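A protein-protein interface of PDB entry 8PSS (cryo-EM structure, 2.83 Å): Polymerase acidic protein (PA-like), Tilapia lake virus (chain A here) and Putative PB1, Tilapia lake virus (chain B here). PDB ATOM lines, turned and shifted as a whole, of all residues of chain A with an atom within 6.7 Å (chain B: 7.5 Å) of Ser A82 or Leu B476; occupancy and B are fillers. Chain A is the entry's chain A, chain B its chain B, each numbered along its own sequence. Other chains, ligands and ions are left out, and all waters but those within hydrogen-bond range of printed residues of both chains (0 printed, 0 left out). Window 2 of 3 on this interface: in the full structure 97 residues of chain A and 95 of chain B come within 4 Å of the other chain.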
ATOM      1  N   VAL A  69       9.755 -22.313  -9.858  1.00  0.00           N
ATOM      2  CA  VAL A  69       8.914 -22.858 -10.916  1.00  0.00           C
ATOM      3  C   VAL A  69       8.109 -24.021 -10.353  1.00  0.00           C
ATOM      4  O   VAL A  69       8.664 -24.930  -9.724  1.00  0.00           O
ATOM      5  CB  VAL A  69       9.762 -23.300 -12.117  1.00  0.00           C
ATOM      6  CG1 VAL A  69       8.886 -23.942 -13.182  1.00  0.00           C
ATOM      7  CG2 VAL A  69      10.523 -22.119 -12.691  1.00  0.00           C
ATOM      8  N   ARG A  70       6.798 -23.995 -10.574  1.00  0.00           N
ATOM      9  CA  ARG A  70       5.894 -25.005 -10.045  1.00  0.00           C
ATOM     10  C   ARG A  70       5.449 -25.942 -11.159  1.00  0.00           C
ATOM     11  O   ARG A  70       5.071 -25.490 -12.245  1.00  0.00           O
ATOM     12  CB  ARG A  70       4.675 -24.355  -9.390  1.00  0.00           C
ATOM     13  CG  ARG A  70       5.011 -23.294  -8.353  1.00  0.00           C
ATOM     14  CD  ARG A  70       5.815 -23.871  -7.200  1.00  0.00           C
ATOM     15  NE  ARG A  70       5.367 -23.367  -5.908  1.00  0.00           N
ATOM     16  CZ  ARG A  70       5.555 -22.129  -5.473  1.00  0.00           C
ATOM     17  NH1 ARG A  70       6.186 -21.225  -6.205  1.00  0.00           N
ATOM     18  NH2 ARG A  70       5.096 -21.787  -4.273  1.00  0.00           N
ATOM     19  N   CYS A  71       5.495 -27.242 -10.884  1.00  0.00           N
ATOM     20  CA  CYS A  71       5.018 -28.269 -11.801  1.00  0.00           C
ATOM     21  C   CYS A  71       3.834 -28.988 -11.169  1.00  0.00           C
ATOM     22  O   CYS A  71       3.931 -29.477 -10.039  1.00  0.00           O
ATOM     23  CB  CYS A  71       6.130 -29.267 -12.131  1.00  0.00           C
ATOM     24  SG  CYS A  71       5.738 -30.390 -13.490  1.00  0.00           S
ATOM     25  N   VAL A  80       1.428 -30.252 -16.038  1.00  0.00           N
ATOM     26  CA  VAL A  80       1.355 -28.835 -16.381  1.00  0.00           C
ATOM     27  C   VAL A  80       2.452 -28.101 -15.625  1.00  0.00           C
ATOM     28  O   VAL A  80       2.673 -28.343 -14.435  1.00  0.00           O
ATOM     29  CB  VAL A  80      -0.037 -28.252 -16.053  1.00  0.00           C
ATOM     30  CG1 VAL A  80       0.033 -26.738 -15.891  1.00  0.00           C
ATOM     31  CG2 VAL A  80      -1.037 -28.642 -17.128  1.00  0.00           C
ATOM     32  N   CYS A  81       3.139 -27.199 -16.322  1.00  0.00           N
ATOM     33  CA  CYS A  81       4.177 -26.385 -15.703  1.00  0.00           C
ATOM     34  C   CYS A  81       4.367 -25.127 -16.538  1.00  0.00           C
ATOM     35  O   CYS A  81       3.782 -24.975 -17.613  1.00  0.00           O
ATOM     36  CB  CYS A  81       5.491 -27.158 -15.567  1.00  0.00           C
ATOM     37  SG  CYS A  81       6.955 -26.102 -15.515  1.00  0.00           S
ATOM     38  N   SER A  82       5.200 -24.221 -16.025  1.00  0.00           N
ATOM     39  CA  SER A  82       5.396 -22.928 -16.673  1.00  0.00           C
ATOM     40  C   SER A  82       6.215 -23.061 -17.953  1.00  0.00           C
ATOM     41  O   SER A  82       5.732 -22.749 -19.046  1.00  0.00           O
ATOM     42  CB  SER A  82       6.074 -21.956 -15.702  1.00  0.00           C
ATOM     43  OG  SER A  82       6.877 -21.019 -16.400  1.00  0.00           O
ATOM     44  N   GLU A  83       7.456 -23.523 -17.835  1.00  0.00           N
ATOM     45  CA  GLU A  83       8.335 -23.627 -18.991  1.00  0.00           C
ATOM     46  C   GLU A  83       7.909 -24.781 -19.888  1.00  0.00           C
ATOM     47  O   GLU A  83       7.503 -25.844 -19.410  1.00  0.00           O
ATOM     48  CB  GLU A  83       9.786 -23.819 -18.547  1.00  0.00           C
ATOM     49  CG  GLU A  83      10.275 -22.788 -17.543  1.00  0.00           C
ATOM     50  CD  GLU A  83      10.263 -21.377 -18.101  1.00  0.00           C
ATOM     51  OE1 GLU A  83      10.193 -21.226 -19.339  1.00  0.00           O
ATOM     52  OE2 GLU A  83      10.325 -20.420 -17.303  1.00  0.00           O
ATOM     53  N   GLN A  84       8.007 -24.562 -21.201  1.00  0.00           N
ATOM     54  CA  GLN A  84       7.655 -25.611 -22.152  1.00  0.00           C
ATOM     55  C   GLN A  84       8.568 -26.820 -22.003  1.00  0.00           C
ATOM     56  O   GLN A  84       8.107 -27.967 -22.053  1.00  0.00           O
ATOM     57  CB  GLN A  84       7.720 -25.065 -23.578  1.00  0.00           C
ATOM     58  CG  GLN A  84       6.879 -25.840 -24.578  1.00  0.00           C
ATOM     59  CD  GLN A  84       7.392 -25.706 -25.998  1.00  0.00           C
ATOM     60  OE1 GLN A  84       7.100 -24.729 -26.687  1.00  0.00           O
ATOM     61  NE2 GLN A  84       8.165 -26.690 -26.443  1.00  0.00           N
ATOM     62  N   GLU A  85       9.870 -26.586 -21.819  1.00  0.00           N
ATOM     63  CA  GLU A  85      10.809 -27.695 -21.700  1.00  0.00           C
ATOM     64  C   GLU A  85      10.489 -28.561 -20.488  1.00  0.00           C
ATOM     65  O   GLU A  85      10.496 -29.794 -20.578  1.00  0.00           O
ATOM     66  CB  GLU A  85      12.240 -27.160 -21.617  1.00  0.00           C
ATOM     67  CG  GLU A  85      13.299 -28.230 -21.384  1.00  0.00           C
ATOM     68  CD  GLU A  85      13.272 -29.320 -22.437  1.00  0.00           C
ATOM     69  OE1 GLU A  85      12.807 -29.049 -23.565  1.00  0.00           O
ATOM     70  OE2 GLU A  85      13.715 -30.449 -22.140  1.00  0.00           O
ATOM     71  N   TYR A  86      10.205 -27.935 -19.344  1.00  0.00           N
ATOM     72  CA  TYR A  86       9.872 -28.705 -18.150  1.00  0.00           C
ATOM     73  C   TYR A  86       8.596 -29.511 -18.355  1.00  0.00           C
ATOM     74  O   TYR A  86       8.511 -30.673 -17.942  1.00  0.00           O
ATOM     75  CB  TYR A  86       9.723 -27.777 -16.944  1.00  0.00           C
ATOM     76  CG  TYR A  86      10.946 -26.947 -16.620  1.00  0.00           C
ATOM     77  CD1 TYR A  86      12.204 -27.302 -17.089  1.00  0.00           C
ATOM     78  CD2 TYR A  86      10.841 -25.810 -15.828  1.00  0.00           C
ATOM     79  CE1 TYR A  86      13.319 -26.542 -16.788  1.00  0.00           C
ATOM     80  CE2 TYR A  86      11.948 -25.047 -15.522  1.00  0.00           C
ATOM     81  CZ  TYR A  86      13.185 -25.417 -16.003  1.00  0.00           C
ATOM     82  OH  TYR A  86      14.289 -24.655 -15.697  1.00  0.00           O
ATOM     83  N   GLN A  87       7.585 -28.907 -18.986  1.00  0.00           N
ATOM     84  CA  GLN A  87       6.343 -29.628 -19.238  1.00  0.00           C
ATOM     85  C   GLN A  87       6.580 -30.818 -20.158  1.00  0.00           C
ATOM     86  O   GLN A  87       6.045 -31.909 -19.925  1.00  0.00           O
ATOM     87  CB  GLN A  87       5.305 -28.679 -19.839  1.00  0.00           C
ATOM     88  CG  GLN A  87       3.925 -29.291 -20.034  1.00  0.00           C
ATOM     89  CD  GLN A  87       3.219 -28.752 -21.262  1.00  0.00           C
ATOM     90  OE1 GLN A  87       3.293 -27.560 -21.561  1.00  0.00           O
ATOM     91  NE2 GLN A  87       2.529 -29.629 -21.982  1.00  0.00           N
ATOM     92  N   LEU B 471       0.323 -25.059 -27.270  1.00  0.00           N
ATOM     93  CA  LEU B 471       1.192 -25.744 -26.322  1.00  0.00           C
ATOM     94  C   LEU B 471       0.987 -25.298 -24.881  1.00  0.00           C
ATOM     95  O   LEU B 471       1.532 -25.935 -23.974  1.00  0.00           O
ATOM     96  CB  LEU B 471       2.660 -25.538 -26.712  1.00  0.00           C
ATOM     97  CG  LEU B 471       3.186 -26.289 -27.941  1.00  0.00           C
ATOM     98  CD1 LEU B 471       3.488 -27.735 -27.581  1.00  0.00           C
ATOM     99  CD2 LEU B 471       2.218 -26.232 -29.113  1.00  0.00           C
ATOM    100  N   VAL B 472       0.224 -24.235 -24.643  1.00  0.00           N
ATOM    101  CA  VAL B 472       0.006 -23.734 -23.289  1.00  0.00           C
ATOM    102  C   VAL B 472      -1.174 -24.476 -22.668  1.00  0.00           C
ATOM    103  O   VAL B 472      -2.296 -24.389 -23.188  1.00  0.00           O
ATOM    104  CB  VAL B 472      -0.236 -22.217 -23.282  1.00  0.00           C
ATOM    105  CG1 VAL B 472      -0.207 -21.688 -21.859  1.00  0.00           C
ATOM    106  CG2 VAL B 472       0.810 -21.508 -24.124  1.00  0.00           C
ATOM    107  N   PRO B 473      -0.981 -25.209 -21.573  1.00  0.00           N
ATOM    108  CA  PRO B 473      -2.123 -25.862 -20.923  1.00  0.00           C
ATOM    109  C   PRO B 473      -3.101 -24.845 -20.360  1.00  0.00           C
ATOM    110  O   PRO B 473      -2.731 -23.733 -19.979  1.00  0.00           O
ATOM    111  CB  PRO B 473      -1.479 -26.690 -19.806  1.00  0.00           C
ATOM    112  CG  PRO B 473      -0.030 -26.769 -20.147  1.00  0.00           C
ATOM    113  CD  PRO B 473       0.287 -25.523 -20.896  1.00  0.00           C
ATOM    114  N   HIS B 474      -4.369 -25.244 -20.309  1.00  0.00           N
ATOM    115  CA  HIS B 474      -5.418 -24.383 -19.781  1.00  0.00           C
ATOM    116  C   HIS B 474      -5.476 -24.385 -18.260  1.00  0.00           C
ATOM    117  O   HIS B 474      -6.237 -23.599 -17.687  1.00  0.00           O
ATOM    118  CB  HIS B 474      -6.775 -24.805 -20.348  1.00  0.00           C
ATOM    119  CG  HIS B 474      -7.025 -24.316 -21.741  1.00  0.00           C
ATOM    120  ND1 HIS B 474      -6.065 -23.664 -22.483  1.00  0.00           N
ATOM    121  CD2 HIS B 474      -8.126 -24.382 -22.524  1.00  0.00           C
ATOM    122  CE1 HIS B 474      -6.563 -23.350 -23.666  1.00  0.00           C
ATOM    123  NE2 HIS B 474      -7.813 -23.774 -23.716  1.00  0.00           N
ATOM    124  N   ARG B 475      -4.699 -25.238 -17.596  1.00  0.00           N
ATOM    125  CA  ARG B 475      -4.613 -25.253 -16.143  1.00  0.00           C
ATOM    126  C   ARG B 475      -3.480 -24.380 -15.619  1.00  0.00           C
ATOM    127  O   ARG B 475      -3.287 -24.294 -14.403  1.00  0.00           O
ATOM    128  CB  ARG B 475      -4.440 -26.687 -15.640  1.00  0.00           C
ATOM    129  CG  ARG B 475      -5.753 -27.400 -15.357  1.00  0.00           C
ATOM    130  CD  ARG B 475      -5.683 -28.881 -15.692  1.00  0.00           C
ATOM    131  NE  ARG B 475      -6.308 -29.700 -14.659  1.00  0.00           N
ATOM    132  CZ  ARG B 475      -7.585 -30.060 -14.650  1.00  0.00           C
ATOM    133  NH1 ARG B 475      -8.421 -29.681 -15.603  1.00  0.00           N
ATOM    134  NH2 ARG B 475      -8.036 -30.818 -13.655  1.00  0.00           N
ATOM    135  N   LEU B 476      -2.731 -23.733 -16.507  1.00  0.00           N
ATOM    136  CA  LEU B 476      -1.631 -22.873 -16.096  1.00  0.00           C
ATOM    137  C   LEU B 476      -2.170 -21.624 -15.411  1.00  0.00           C
ATOM    138  O   LEU B 476      -3.120 -21.000 -15.892  1.00  0.00           O
ATOM    139  CB  LEU B 476      -0.786 -22.489 -17.310  1.00  0.00           C
ATOM    140  CG  LEU B 476       0.470 -21.667 -17.022  1.00  0.00           C
ATOM    141  CD1 LEU B 476       1.709 -22.525 -17.167  1.00  0.00           C
ATOM    142  CD2 LEU B 476       0.541 -20.463 -17.946  1.00  0.00           C
ATOM    143  N   LEU B 477      -1.562 -21.264 -14.284  1.00  0.00           N
ATOM    144  CA  LEU B 477      -1.969 -20.078 -13.545  1.00  0.00           C
ATOM    145  C   LEU B 477      -1.362 -18.835 -14.182  1.00  0.00           C
ATOM    146  O   LEU B 477      -0.178 -18.819 -14.528  1.00  0.00           O
ATOM    147  CB  LEU B 477      -1.537 -20.187 -12.084  1.00  0.00           C
ATOM    148  CG  LEU B 477      -2.543 -20.856 -11.148  1.00  0.00           C
ATOM    149  CD1 LEU B 477      -2.765 -22.303 -11.552  1.00  0.00           C
ATOM    150  CD2 LEU B 477      -2.074 -20.763  -9.707  1.00  0.00           C
ATOM    151  N   VAL B 478      -2.176 -17.792 -14.335  1.00  0.00           N
ATOM    152  CA  VAL B 478      -1.738 -16.539 -14.934  1.00  0.00           C
ATOM    153  C   VAL B 478      -2.222 -15.380 -14.076  1.00  0.00           C
ATOM    154  O   VAL B 478      -3.212 -15.490 -13.348  1.00  0.00           O
ATOM    155  CB  VAL B 478      -2.248 -16.385 -16.385  1.00  0.00           C
ATOM    156  CG1 VAL B 478      -1.659 -17.468 -17.270  1.00  0.00           C
ATOM    157  CG2 VAL B 478      -3.769 -16.420 -16.425  1.00  0.00           C
ATOM    158  N   SER B 479      -1.510 -14.263 -14.168  1.00  0.00           N
ATOM    159  CA  SER B 479      -1.869 -13.016 -13.512  1.00  0.00           C
ATOM    160  C   SER B 479      -2.178 -11.958 -14.568  1.00  0.00           C
ATOM    161  O   SER B 479      -2.100 -12.208 -15.775  1.00  0.00           O
ATOM    162  CB  SER B 479      -0.745 -12.558 -12.579  1.00  0.00           C
ATOM    163  OG  SER B 479       0.526 -12.872 -13.122  1.00  0.00           O
ATOM    164  N   ASP B 482       0.776 -11.336 -16.739  1.00  0.00           N
ATOM    165  CA  ASP B 482       1.014 -12.444 -17.658  1.00  0.00           C
ATOM    166  C   ASP B 482       0.099 -12.357 -18.873  1.00  0.00           C
ATOM    167  O   ASP B 482       0.553 -12.484 -20.016  1.00  0.00           O
ATOM    168  CB  ASP B 482       0.815 -13.774 -16.935  1.00  0.00           C
ATOM    169  CG  ASP B 482       1.998 -14.148 -16.067  1.00  0.00           C
ATOM    170  OD1 ASP B 482       3.073 -14.455 -16.624  1.00  0.00           O
ATOM    171  OD2 ASP B 482       1.854 -14.137 -14.826  1.00  0.00           O
ATOM    172  N   ILE B 486       1.064 -11.930 -22.844  1.00  0.00           N
ATOM    173  CA  ILE B 486       0.640 -12.861 -23.889  1.00  0.00           C
ATOM    174  C   ILE B 486      -0.087 -12.110 -24.997  1.00  0.00           C
ATOM    175  O   ILE B 486       0.190 -12.302 -26.188  1.00  0.00           O
ATOM    176  CB  ILE B 486      -0.235 -13.982 -23.298  1.00  0.00           C
ATOM    177  CG1 ILE B 486       0.524 -14.717 -22.188  1.00  0.00           C
ATOM    178  CG2 ILE B 486      -0.678 -14.958 -24.393  1.00  0.00           C
ATOM    179  CD1 ILE B 486       0.066 -16.141 -21.942  1.00  0.00           C
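Ser A82 touches just one residue of chain B: Leu B476. Printed residues of chain B within 4 Å of Gln A87: Leu B471 (3.4 Å) and Pro B473 (3.7 Å). Printed residues of chain A within 4 Å of Leu B471: Gln A87 (3.4 Å). Leu B476 touches two residues of chain A. The nearest residue of chain B that does not touch Ser A82 is Pro B473 (6.4 Å). The nearest printed residue of chain B that does not touch Gln A87 is Val B472 (5.3 Å).
The backbone carbonyl oxygen (O) of Leu B471 sits close to the side-chain amide oxygen (OE1) of Gln A87, 3.4 Å away.
Along chain B the printed residues that touch a printed residue of chain A span positions 471 to 476. Of the 11 printed residues of chain A, 4 touch a printed residue of chain B. Printed residues of chain A that touch a printed residue of chain B: Val A80, Cys A81, Ser A82 and Gln A87. Along chain A the printed residues that touch a printed residue of chain B span positions 80 to 87.
Val A80 touches Pro B473 (CG2 to CB, 3.3 Å). Cys A81 touches Leu B476. Ser A82 touches Leu B476. Pro B473 touches Gln A87.
SG of Cys A81 lies within hydrogen-bond range of N of Glu A83 (3.5 Å).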
